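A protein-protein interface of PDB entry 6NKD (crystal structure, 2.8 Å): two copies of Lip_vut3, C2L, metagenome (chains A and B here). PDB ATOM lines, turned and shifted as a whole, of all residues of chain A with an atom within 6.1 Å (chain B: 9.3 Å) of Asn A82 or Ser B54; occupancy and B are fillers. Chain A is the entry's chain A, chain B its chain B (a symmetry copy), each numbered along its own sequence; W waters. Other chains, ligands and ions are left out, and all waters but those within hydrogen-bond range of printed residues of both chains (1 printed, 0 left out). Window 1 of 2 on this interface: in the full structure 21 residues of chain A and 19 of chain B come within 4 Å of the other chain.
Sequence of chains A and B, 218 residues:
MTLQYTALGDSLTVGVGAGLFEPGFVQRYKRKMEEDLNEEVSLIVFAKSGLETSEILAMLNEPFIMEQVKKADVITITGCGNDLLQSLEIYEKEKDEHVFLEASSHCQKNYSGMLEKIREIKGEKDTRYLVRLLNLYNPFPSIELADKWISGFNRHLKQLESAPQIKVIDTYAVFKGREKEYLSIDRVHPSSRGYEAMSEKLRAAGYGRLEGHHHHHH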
ATOM      1  N   ASP A  10     -16.467  32.696  21.836  1.00  0.00           N
ATOM      2  CA  ASP A  10     -17.389  31.985  22.710  1.00  0.00           C
ATOM      3  C   ASP A  10     -17.700  32.792  23.963  1.00  0.00           C
ATOM      4  O   ASP A  10     -17.951  33.999  23.885  1.00  0.00           O
ATOM      5  CB  ASP A  10     -16.811  30.613  23.073  1.00  0.00           C
ATOM      6  CG  ASP A  10     -15.392  30.697  23.619  1.00  0.00           C
ATOM      7  OD1 ASP A  10     -14.864  29.655  24.064  1.00  0.00           O
ATOM      8  OD2 ASP A  10     -14.812  31.804  23.621  1.00  0.00           O
ATOM      9  N   SER A  49     -22.232  31.688  24.262  1.00  0.00           N
ATOM     10  CA  SER A  49     -21.687  30.558  25.003  1.00  0.00           C
ATOM     11  C   SER A  49     -21.924  29.259  24.240  1.00  0.00           C
ATOM     12  O   SER A  49     -22.996  29.040  23.669  1.00  0.00           O
ATOM     13  CB  SER A  49     -22.319  30.482  26.393  1.00  0.00           C
ATOM     14  OG  SER A  49     -22.000  31.635  27.150  1.00  0.00           O
ATOM     15  N   GLY A  50     -20.910  28.399  24.224  1.00  0.00           N
ATOM     16  CA  GLY A  50     -20.998  27.147  23.502  1.00  0.00           C
ATOM     17  C   GLY A  50     -20.837  27.257  22.005  1.00  0.00           C
ATOM     18  O   GLY A  50     -21.176  26.307  21.291  1.00  0.00           O
ATOM     19  N   LEU A  51     -20.334  28.381  21.502  1.00  0.00           N
ATOM     20  CA  LEU A  51     -20.115  28.559  20.069  1.00  0.00           C
ATOM     21  C   LEU A  51     -18.758  27.965  19.719  1.00  0.00           C
ATOM     22  O   LEU A  51     -17.715  28.578  19.961  1.00  0.00           O
ATOM     23  CB  LEU A  51     -20.192  30.034  19.692  1.00  0.00           C
ATOM     24  CG  LEU A  51     -20.999  30.369  18.437  1.00  0.00           C
ATOM     25  CD1 LEU A  51     -22.455  29.974  18.626  1.00  0.00           C
ATOM     26  CD2 LEU A  51     -20.879  31.848  18.105  1.00  0.00           C
ATOM     27  N   GLU A  52     -18.764  26.764  19.147  1.00  0.00           N
ATOM     28  CA  GLU A  52     -17.523  26.082  18.825  1.00  0.00           C
ATOM     29  C   GLU A  52     -16.889  26.682  17.570  1.00  0.00           C
ATOM     30  O   GLU A  52     -17.481  27.508  16.869  1.00  0.00           O
ATOM     31  CB  GLU A  52     -17.766  24.583  18.660  1.00  0.00           C
ATOM     32  CG  GLU A  52     -18.315  23.924  19.918  1.00  0.00           C
ATOM     33  CD  GLU A  52     -18.284  22.410  19.856  1.00  0.00           C
ATOM     34  OE1 GLU A  52     -17.634  21.862  18.941  1.00  0.00           O
ATOM     35  OE2 GLU A  52     -18.908  21.767  20.728  1.00  0.00           O
ATOM     36  N   GLY A  79     -12.045  30.620  21.157  1.00  0.00           N
ATOM     37  CA  GLY A  79     -12.726  29.367  20.899  1.00  0.00           C
ATOM     38  C   GLY A  79     -11.930  28.191  21.415  1.00  0.00           C
ATOM     39  O   GLY A  79     -10.829  28.337  21.958  1.00  0.00           O
ATOM     40  N   CYS A  80     -12.526  27.011  21.237  1.00  0.00           N
ATOM     41  CA  CYS A  80     -12.010  25.694  21.605  1.00  0.00           C
ATOM     42  C   CYS A  80     -11.903  25.491  23.113  1.00  0.00           C
ATOM     43  O   CYS A  80     -11.456  24.421  23.544  1.00  0.00           O
ATOM     44  CB  CYS A  80     -10.644  25.402  20.966  1.00  0.00           C
ATOM     45  SG  CYS A  80     -10.303  23.657  20.643  1.00  0.00           S
ATOM     46  N   GLY A  81     -12.304  26.469  23.928  1.00  0.00           N
ATOM     47  CA  GLY A  81     -12.241  26.288  25.370  1.00  0.00           C
ATOM     48  C   GLY A  81     -13.205  25.232  25.881  1.00  0.00           C
ATOM     49  O   GLY A  81     -12.881  24.479  26.804  1.00  0.00           O
ATOM     50  N   ASN A  82     -14.403  25.163  25.297  1.00  0.00           N
ATOM     51  CA  ASN A  82     -15.383  24.179  25.743  1.00  0.00           C
ATOM     52  C   ASN A  82     -15.053  22.774  25.258  1.00  0.00           C
ATOM     53  O   ASN A  82     -15.503  21.798  25.870  1.00  0.00           O
ATOM     54  CB  ASN A  82     -16.782  24.586  25.279  1.00  0.00           C
ATOM     55  CG  ASN A  82     -17.874  23.757  25.924  1.00  0.00           C
ATOM     56  OD1 ASN A  82     -18.541  22.963  25.260  1.00  0.00           O
ATOM     57  ND2 ASN A  82     -18.060  23.935  27.227  1.00  0.00           N
ATOM     58  N   ASP A  83     -14.282  22.647  24.174  1.00  0.00           N
ATOM     59  CA  ASP A  83     -13.851  21.326  23.731  1.00  0.00           C
ATOM     60  C   ASP A  83     -12.932  20.669  24.752  1.00  0.00           C
ATOM     61  O   ASP A  83     -12.945  19.442  24.900  1.00  0.00           O
ATOM     62  CB  ASP A  83     -13.152  21.425  22.374  1.00  0.00           C
ATOM     63  CG  ASP A  83     -14.023  22.070  21.314  1.00  0.00           C
ATOM     64  OD1 ASP A  83     -15.058  22.669  21.674  1.00  0.00           O
ATOM     65  OD2 ASP A  83     -13.674  21.975  20.118  1.00  0.00           O
ATOM     66  N   LEU A  84     -12.131  21.469  25.462  1.00  0.00           N
ATOM     67  CA  LEU A  84     -11.290  20.922  26.521  1.00  0.00           C
ATOM     68  C   LEU A  84     -12.140  20.357  27.650  1.00  0.00           C
ATOM     69  O   LEU A  84     -11.851  19.272  28.172  1.00  0.00           O
ATOM     70  CB  LEU A  84     -10.337  22.004  27.036  1.00  0.00           C
ATOM     71  CG  LEU A  84      -9.266  21.673  28.084  1.00  0.00           C
ATOM     72  CD1 LEU A  84      -9.793  21.815  29.511  1.00  0.00           C
ATOM     73  CD2 LEU A  84      -8.678  20.284  27.862  1.00  0.00           C
ATOM     74  N   LEU A  85     -13.195  21.076  28.042  1.00  0.00           N
ATOM     75  CA  LEU A  85     -14.081  20.577  29.088  1.00  0.00           C
ATOM     76  C   LEU A  85     -14.782  19.299  28.649  1.00  0.00           C
ATOM     77  O   LEU A  85     -14.898  18.348  29.430  1.00  0.00           O
ATOM     78  CB  LEU A  85     -15.105  21.647  29.470  1.00  0.00           C
ATOM     79  CG  LEU A  85     -14.751  22.593  30.624  1.00  0.00           C
ATOM     80  CD1 LEU A  85     -13.502  23.403  30.317  1.00  0.00           C
ATOM     81  CD2 LEU A  85     -15.922  23.513  30.944  1.00  0.00           C
ATOM     82  N   GLN A  86     -15.254  19.256  27.401  1.00  0.00           N
ATOM     83  CA  GLN A  86     -15.888  18.042  26.897  1.00  0.00           C
ATOM     84  C   GLN A  86     -14.895  16.889  26.837  1.00  0.00           C
ATOM     85  O   GLN A  86     -15.239  15.746  27.158  1.00  0.00           O
ATOM     86  CB  GLN A  86     -16.495  18.296  25.517  1.00  0.00           C
ATOM     87  CG  GLN A  86     -17.676  19.252  25.511  1.00  0.00           C
ATOM     88  CD  GLN A  86     -18.224  19.479  24.115  1.00  0.00           C
ATOM     89  OE1 GLN A  86     -17.675  18.979  23.134  1.00  0.00           O
ATOM     90  NE2 GLN A  86     -19.312  20.234  24.021  1.00  0.00           N
ATOM     91  N   SER A  87     -13.654  17.171  26.434  1.00  0.00           N
ATOM     92  CA  SER A  87     -12.661  16.109  26.302  1.00  0.00           C
ATOM     93  C   SER A  87     -12.244  15.562  27.661  1.00  0.00           C
ATOM     94  O   SER A  87     -12.042  14.351  27.811  1.00  0.00           O
ATOM     95  CB  SER A  87     -11.445  16.620  25.531  1.00  0.00           C
ATOM     96  OG  SER A  87     -11.797  16.976  24.207  1.00  0.00           O
ATOM     97  N   HIS A 189     -14.295  29.912  34.006  1.00  0.00           N
ATOM     98  CA  HIS A 189     -14.356  31.177  33.292  1.00  0.00           C
ATOM     99  C   HIS A 189     -13.589  32.256  34.048  1.00  0.00           C
ATOM    100  O   HIS A 189     -13.495  32.213  35.278  1.00  0.00           O
ATOM    101  CB  HIS A 189     -15.810  31.619  33.092  1.00  0.00           C
ATOM    102  CG  HIS A 189     -16.524  30.859  32.020  1.00  0.00           C
ATOM    103  ND1 HIS A 189     -17.374  29.807  32.288  1.00  0.00           N
ATOM    104  CD2 HIS A 189     -16.501  30.986  30.672  1.00  0.00           C
ATOM    105  CE1 HIS A 189     -17.850  29.326  31.154  1.00  0.00           C
ATOM    106  NE2 HIS A 189     -17.335  30.025  30.157  1.00  0.00           N
ATOM    107  N   GLY B  50     -32.688  30.941  27.896  1.00  0.00           N
ATOM    108  CA  GLY B  50     -31.586  30.902  26.957  1.00  0.00           C
ATOM    109  C   GLY B  50     -30.282  30.395  27.525  1.00  0.00           C
ATOM    110  O   GLY B  50     -29.229  30.619  26.923  1.00  0.00           O
ATOM    111  N   LEU B  51     -30.317  29.718  28.670  1.00  0.00           N
ATOM    112  CA  LEU B  51     -29.096  29.191  29.265  1.00  0.00           C
ATOM    113  C   LEU B  51     -28.535  28.067  28.404  1.00  0.00           C
ATOM    114  O   LEU B  51     -29.237  27.101  28.086  1.00  0.00           O
ATOM    115  CB  LEU B  51     -29.367  28.693  30.682  1.00  0.00           C
ATOM    116  CG  LEU B  51     -28.159  28.169  31.460  1.00  0.00           C
ATOM    117  CD1 LEU B  51     -27.089  29.245  31.571  1.00  0.00           C
ATOM    118  CD2 LEU B  51     -28.578  27.679  32.837  1.00  0.00           C
ATOM    119  N   GLU B  52     -27.266  28.194  28.025  1.00  0.00           N
ATOM    120  CA  GLU B  52     -26.627  27.214  27.163  1.00  0.00           C
ATOM    121  C   GLU B  52     -26.246  25.961  27.946  1.00  0.00           C
ATOM    122  O   GLU B  52     -26.091  25.979  29.170  1.00  0.00           O
ATOM    123  CB  GLU B  52     -25.386  27.812  26.500  1.00  0.00           C
ATOM    124  CG  GLU B  52     -25.690  28.727  25.330  1.00  0.00           C
ATOM    125  CD  GLU B  52     -26.271  27.979  24.143  1.00  0.00           C
ATOM    126  OE1 GLU B  52     -27.147  28.544  23.454  1.00  0.00           O
ATOM    127  OE2 GLU B  52     -25.854  26.825  23.901  1.00  0.00           O
ATOM    128  N   THR B  53     -26.096  24.855  27.212  1.00  0.00           N
ATOM    129  CA  THR B  53     -25.665  23.609  27.836  1.00  0.00           C
ATOM    130  C   THR B  53     -24.192  23.650  28.215  1.00  0.00           C
ATOM    131  O   THR B  53     -23.795  23.039  29.213  1.00  0.00           O
ATOM    132  CB  THR B  53     -25.934  22.426  26.906  1.00  0.00           C
ATOM    133  OG1 THR B  53     -25.603  22.785  25.559  1.00  0.00           O
ATOM    134  CG2 THR B  53     -27.390  22.012  26.987  1.00  0.00           C
ATOM    135  N   SER B  54     -23.371  24.354  27.434  1.00  0.00           N
ATOM    136  CA  SER B  54     -21.968  24.509  27.802  1.00  0.00           C
ATOM    137  C   SER B  54     -21.821  25.263  29.116  1.00  0.00           C
ATOM    138  O   SER B  54     -20.874  25.019  29.871  1.00  0.00           O
ATOM    139  CB  SER B  54     -21.208  25.226  26.688  1.00  0.00           C
ATOM    140  OG  SER B  54     -21.759  26.508  26.452  1.00  0.00           O
ATOM    141  N   GLU B  55     -22.752  26.175  29.410  1.00  0.00           N
ATOM    142  CA  GLU B  55     -22.699  26.895  30.676  1.00  0.00           C
ATOM    143  C   GLU B  55     -23.023  25.973  31.845  1.00  0.00           C
ATOM    144  O   GLU B  55     -22.436  26.103  32.925  1.00  0.00           O
ATOM    145  CB  GLU B  55     -23.660  28.080  30.650  1.00  0.00           C
ATOM    146  CG  GLU B  55     -23.185  29.264  31.469  1.00  0.00           C
ATOM    147  CD  GLU B  55     -22.216  30.139  30.701  1.00  0.00           C
ATOM    148  OE1 GLU B  55     -22.682  30.998  29.922  1.00  0.00           O
ATOM    149  OE2 GLU B  55     -20.989  29.960  30.864  1.00  0.00           O
ATOM    150  N   ILE B  56     -23.956  25.038  31.649  1.00  0.00           N
ATOM    151  CA  ILE B  56     -24.318  24.108  32.715  1.00  0.00           C
ATOM    152  C   ILE B  56     -23.126  23.238  33.088  1.00  0.00           C
ATOM    153  O   ILE B  56     -22.859  23.000  34.272  1.00  0.00           O
ATOM    154  CB  ILE B  56     -25.529  23.255  32.292  1.00  0.00           C
ATOM    155  CG1 ILE B  56     -26.713  24.149  31.926  1.00  0.00           C
ATOM    156  CG2 ILE B  56     -25.912  22.299  33.404  1.00  0.00           C
ATOM    157  CD1 ILE B  56     -27.960  23.382  31.543  1.00  0.00           C
ATOM    158  N   LEU B  57     -22.392  22.752  32.084  1.00  0.00           N
ATOM    159  CA  LEU B  57     -21.193  21.967  32.353  1.00  0.00           C
ATOM    160  C   LEU B  57     -20.173  22.770  33.149  1.00  0.00           C
ATOM    161  O   LEU B  57     -19.421  22.202  33.950  1.00  0.00           O
ATOM    162  CB  LEU B  57     -20.585  21.479  31.038  1.00  0.00           C
ATOM    163  CG  LEU B  57     -19.357  20.576  31.130  1.00  0.00           C
ATOM    164  CD1 LEU B  57     -19.666  19.341  31.960  1.00  0.00           C
ATOM    165  CD2 LEU B  57     -18.879  20.188  29.739  1.00  0.00           C
ATOM    166  N   ALA B  58     -20.142  24.088  32.956  1.00  0.00           N
ATOM    167  CA  ALA B  58     -19.246  24.940  33.729  1.00  0.00           C
ATOM    168  C   ALA B  58     -19.806  25.230  35.116  1.00  0.00           C
ATOM    169  O   ALA B  58     -19.043  25.355  36.080  1.00  0.00           O
ATOM    170  CB  ALA B  58     -18.989  26.243  32.976  1.00  0.00           C
ATOM    171  N   MET B  59     -21.128  25.344  35.229  1.00  0.00           N
ATOM    172  CA  MET B  59     -21.791  25.642  36.496  1.00  0.00           C
ATOM    173  C   MET B  59     -21.539  24.576  37.547  1.00  0.00           C
ATOM    174  O   MET B  59     -21.418  24.876  38.736  1.00  0.00           O
ATOM    175  CB  MET B  59     -23.296  25.782  36.290  1.00  0.00           C
ATOM    176  CG  MET B  59     -23.741  27.066  35.633  1.00  0.00           C
ATOM    177  SD  MET B  59     -25.529  26.824  34.912  1.00  0.00           S
ATOM    178  CE  MET B  59     -26.341  25.951  36.454  1.00  0.00           C
ATOM    179  N   LEU B  60     -21.471  23.322  37.097  1.00  0.00           N
ATOM    180  CA  LEU B  60     -21.308  22.196  38.009  1.00  0.00           C
ATOM    181  C   LEU B  60     -20.010  22.262  38.801  1.00  0.00           C
ATOM    182  O   LEU B  60     -19.838  21.479  39.740  1.00  0.00           O
ATOM    183  CB  LEU B  60     -21.385  20.884  37.225  1.00  0.00           C
ATOM    184  CG  LEU B  60     -22.722  20.616  36.524  1.00  0.00           C
ATOM    185  CD1 LEU B  60     -22.632  19.390  35.627  1.00  0.00           C
ATOM    186  CD2 LEU B  60     -23.841  20.453  37.542  1.00  0.00           C
ATOM    187  N   ASN B  61     -19.099  23.169  38.451  1.00  0.00           N
ATOM    188  CA  ASN B  61     -17.904  23.408  39.245  1.00  0.00           C
ATOM    189  C   ASN B  61     -18.117  24.445  40.338  1.00  0.00           C
ATOM    190  O   ASN B  61     -17.263  24.571  41.224  1.00  0.00           O
ATOM    191  CB  ASN B  61     -16.747  23.851  38.346  1.00  0.00           C
ATOM    192  CG  ASN B  61     -16.237  22.735  37.460  1.00  0.00           C
ATOM    193  OD1 ASN B  61     -15.319  22.003  37.833  1.00  0.00           O
ATOM    194  ND2 ASN B  61     -16.826  22.598  36.279  1.00  0.00           N
ATOM    195  N   THR B  78     -33.404  20.550  31.403  1.00  0.00           N
ATOM    196  CA  THR B  78     -33.898  21.028  30.123  1.00  0.00           C
ATOM    197  C   THR B  78     -32.810  21.851  29.446  1.00  0.00           C
ATOM    198  O   THR B  78     -31.849  22.290  30.083  1.00  0.00           O
ATOM    199  CB  THR B  78     -35.168  21.873  30.286  1.00  0.00           C
ATOM    200  OG1 THR B  78     -34.972  22.850  31.315  1.00  0.00           O
ATOM    201  CG2 THR B  78     -36.355  20.992  30.640  1.00  0.00           C
ATOM    202  N   GLY B  79     -32.960  22.049  28.143  1.00  0.00           N
ATOM    203  CA  GLY B  79     -31.978  22.834  27.420  1.00  0.00           C
ATOM    204  C   GLY B  79     -32.097  22.645  25.928  1.00  0.00           C
ATOM    205  O   GLY B  79     -32.790  21.750  25.435  1.00  0.00           O
ATOM    206  N   CYS B  80     -31.405  23.530  25.210  1.00  0.00           N
ATOM    207  CA  CYS B  80     -31.267  23.565  23.757  1.00  0.00           C
ATOM    208  C   CYS B  80     -32.571  23.903  23.047  1.00  0.00           C
ATOM    209  O   CYS B  80     -32.588  23.937  21.811  1.00  0.00           O
ATOM    210  CB  CYS B  80     -30.712  22.248  23.192  1.00  0.00           C
ATOM    211  SG  CYS B  80     -29.341  21.568  24.164  1.00  0.00           S
ATOM    212  N   ASP B  83     -31.915  27.074  21.176  1.00  0.00           N
ATOM    213  CA  ASP B  83     -30.902  27.014  20.127  1.00  0.00           C
ATOM    214  C   ASP B  83     -31.522  26.710  18.768  1.00  0.00           C
ATOM    215  O   ASP B  83     -31.115  27.285  17.752  1.00  0.00           O
ATOM    216  CB  ASP B  83     -29.841  25.973  20.479  1.00  0.00           C
ATOM    217  CG  ASP B  83     -28.881  26.460  21.545  1.00  0.00           C
ATOM    218  OD1 ASP B  83     -29.254  26.448  22.738  1.00  0.00           O
ATOM    219  OD2 ASP B  83     -27.755  26.863  21.187  1.00  0.00           O
ATOM    220  N   SER B 105     -25.178  18.537  17.267  1.00  0.00           N
ATOM    221  CA  SER B 105     -23.755  18.230  17.368  1.00  0.00           C
ATOM    222  C   SER B 105     -23.145  18.759  18.662  1.00  0.00           C
ATOM    223  O   SER B 105     -22.419  18.034  19.351  1.00  0.00           O
ATOM    224  CB  SER B 105     -23.010  18.795  16.157  1.00  0.00           C
ATOM    225  OG  SER B 105     -21.638  18.446  16.195  1.00  0.00           O
ATOM    226  N   HIS B 106     -23.425  20.015  19.009  1.00  0.00           N
ATOM    227  CA  HIS B 106     -22.749  20.654  20.133  1.00  0.00           C
ATOM    228  C   HIS B 106     -23.521  20.563  21.443  1.00  0.00           C
ATOM    229  O   HIS B 106     -22.900  20.563  22.510  1.00  0.00           O
ATOM    230  CB  HIS B 106     -22.457  22.125  19.807  1.00  0.00           C
ATOM    231  CG  HIS B 106     -23.516  23.077  20.268  1.00  0.00           C
ATOM    232  ND1 HIS B 106     -24.754  23.161  19.670  1.00  0.00           N
ATOM    233  CD2 HIS B 106     -23.516  23.994  21.264  1.00  0.00           C
ATOM    234  CE1 HIS B 106     -25.475  24.084  20.282  1.00  0.00           C
ATOM    235  NE2 HIS B 106     -24.747  24.604  21.253  1.00  0.00           N
ATOM    236  N   CYS B 107     -24.851  20.473  21.401  1.00  0.00           N
ATOM    237  CA  CYS B 107     -25.622  20.333  22.632  1.00  0.00           C
ATOM    238  C   CYS B 107     -25.547  18.912  23.180  1.00  0.00           C
ATOM    239  O   CYS B 107     -25.404  18.718  24.393  1.00  0.00           O
ATOM    240  CB  CYS B 107     -27.080  20.729  22.384  1.00  0.00           C
ATOM    241  SG  CYS B 107     -27.653  22.209  23.233  1.00  0.00           S
ATOM    242  N   GLN B 108     -25.631  17.910  22.301  1.00  0.00           N
ATOM    243  CA  GLN B 108     -25.641  16.523  22.755  1.00  0.00           C
ATOM    244  C   GLN B 108     -24.310  16.139  23.391  1.00  0.00           C
ATOM    245  O   GLN B 108     -24.277  15.383  24.368  1.00  0.00           O
ATOM    246  CB  GLN B 108     -25.977  15.599  21.583  1.00  0.00           C
ATOM    247  CG  GLN B 108     -26.711  14.329  21.976  1.00  0.00           C
ATOM    248  CD  GLN B 108     -25.843  13.095  21.858  1.00  0.00           C
ATOM    249  OE1 GLN B 108     -25.199  12.680  22.819  1.00  0.00           O
ATOM    250  NE2 GLN B 108     -25.825  12.498  20.671  1.00  0.00           N
ATOM    251  N   LYS B 109     -23.201  16.658  22.857  1.00  0.00           N
ATOM    252  CA  LYS B 109     -21.901  16.369  23.455  1.00  0.00           C
ATOM    253  C   LYS B 109     -21.734  17.066  24.799  1.00  0.00           C
ATOM    254  O   LYS B 109     -21.062  16.533  25.690  1.00  0.00           O
ATOM    255  CB  LYS B 109     -20.782  16.767  22.495  1.00  0.00           C
ATOM    256  CG  LYS B 109     -20.756  15.931  21.227  1.00  0.00           C
ATOM    257  CD  LYS B 109     -19.493  16.167  20.417  1.00  0.00           C
ATOM    258  CE  LYS B 109     -19.433  15.238  19.213  1.00  0.00           C
ATOM    259  NZ  LYS B 109     -18.150  15.367  18.466  1.00  0.00           N
ATOM    260  N   ASN B 110     -22.332  18.248  24.969  1.00  0.00           N
ATOM    261  CA  ASN B 110     -22.334  18.881  26.283  1.00  0.00           C
ATOM    262  C   ASN B 110     -23.192  18.102  27.273  1.00  0.00           C
ATOM    263  O   ASN B 110     -22.930  18.137  28.481  1.00  0.00           O
ATOM    264  CB  ASN B 110     -22.826  20.326  26.180  1.00  0.00           C
ATOM    265  CG  ASN B 110     -21.743  21.284  25.719  1.00  0.00           C
ATOM    266  OD1 ASN B 110     -21.892  21.967  24.706  1.00  0.00           O
ATOM    267  ND2 ASN B 110     -20.648  21.346  26.470  1.00  0.00           N
ATOM    268  N   TYR B 111     -24.213  17.394  26.784  1.00  0.00           N
ATOM    269  CA  TYR B 111     -25.067  16.608  27.670  1.00  0.00           C
ATOM    270  C   TYR B 111     -24.311  15.422  28.257  1.00  0.00           C
ATOM    271  O   TYR B 111     -24.421  15.136  29.455  1.00  0.00           O
ATOM    272  CB  TYR B 111     -26.310  16.130  26.921  1.00  0.00           C
ATOM    273  CG  TYR B 111     -27.497  17.064  27.015  1.00  0.00           C
ATOM    274  CD1 TYR B 111     -28.055  17.385  28.246  1.00  0.00           C
ATOM    275  CD2 TYR B 111     -28.073  17.604  25.873  1.00  0.00           C
ATOM    276  CE1 TYR B 111     -29.143  18.231  28.338  1.00  0.00           C
ATOM    277  CE2 TYR B 111     -29.162  18.451  25.955  1.00  0.00           C
ATOM    278  CZ  TYR B 111     -29.693  18.762  27.189  1.00  0.00           C
ATOM    279  OH  TYR B 111     -30.778  19.604  27.275  1.00  0.00           O
ATOM    280  N   GLY B 113     -21.069  15.127  28.645  1.00  0.00           N
ATOM    281  CA  GLY B 113     -20.123  15.662  29.606  1.00  0.00           C
ATOM    282  C   GLY B 113     -20.789  16.117  30.888  1.00  0.00           C
ATOM    283  O   GLY B 113     -20.187  16.047  31.965  1.00  0.00           O
ATOM    284  N   MET B 114     -22.028  16.586  30.797  1.00  0.00           N
ATOM    285  CA  MET B 114     -22.818  16.951  31.965  1.00  0.00           C
ATOM    286  C   MET B 114     -23.029  15.745  32.870  1.00  0.00           C
ATOM    287  O   MET B 114     -22.734  15.789  34.065  1.00  0.00           O
ATOM    288  CB  MET B 114     -24.166  17.515  31.527  1.00  0.00           C
ATOM    289  CG  MET B 114     -24.462  18.917  32.003  1.00  0.00           C
ATOM    290  SD  MET B 114     -26.189  19.487  31.313  1.00  0.00           S
ATOM    291  CE  MET B 114     -25.683  19.799  29.457  1.00  0.00           C
HETATM  292  O   HOH W   1     -18.282  26.219  29.140  1.00  0.00           O
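Water W1 lies within hydrogen-bond range of O of Ser B54 (2.9 Å) and ND2 of Asn A82 (3.0 Å).
The side-chain hydroxyl (OG) of Ser A49 is in hydrogen-bond range of the side-chain carboxylate (OE1) of Glu B55. The backbone NH of Gly A50 is in hydrogen-bond range of the side-chain hydroxyl of Ser B54 (3.0 Å). OD1 of Asn A82 sits at hydrogen-bond distance from ND2 of Asn B110 (2.9 Å). The side-chain amide nitrogen of Gln A86 sits close to the side-chain amide nitrogen of Asn B110 (3.0 Å).
The side-chain amide oxygen (OD1) of Asn A82 lies within hydrogen-bond range of the side-chain amide nitrogen (NE2) of Gln A86, 3.1 Å away. OD1 of Asn B110 sits close to O of His B106 (2.8 Å). SG of Cys B80 forms a disulfide with SG of Cys B107 (2.0 Å).
Positions printed for both chains: 50, 51, 52, 79, 80 and 83. Of the 13 pairs that touch across the chains among the printed residues, none has its exchanged pair printed and touching as well.
O of Ser A49 touches CG of Glu B52, at 3.2 Å. Ser B54 touches Ser A49. His B106 touches Gly A50 (CD2 to O, 3.3 Å). CB of His B106 touches OE2 of Glu A52, at 3.7 Å. Asn A82 touches Ser B54 (ND2 to CB, 3.4 Å). His B106 touches Gln A86. Gln A86 touches Lys B109. His A189 touches Glu B55 (CE1 to OE2, 3.2 Å). CE1 of His A189 touches CB of Ala B58, at 3.8 Å.
Of chain B, only Ser B54 (3.0 Å) and His B106 (3.3 Å) come within 4 Å of Gly A50. No residue of chain B comes within 4 Å of Gly A81. Asn A82 touches just these residues of chain B: Ser B54 and Asn B110. Ser B54 touches three residues of chain A. Printed residues of chain A within 4 Å of Glu B55: Ser A49 (2.9 Å) and His A189 (3.2 Å). Of the printed residues of chain A, Ala B58 touches His A189 (3.8 Å). The nearest residue of chain B that does not touch Asn A82 is Leu B57 (4.6 Å).
Hydrophobic or aromatic side chains of chain B within 4 Å of the printed part of chain A: Ala B58 and His B106. Among the printed residues, no Asp or Glu carboxylate lies within 4 Å of a Lys or Arg side-chain nitrogen of the other chain.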
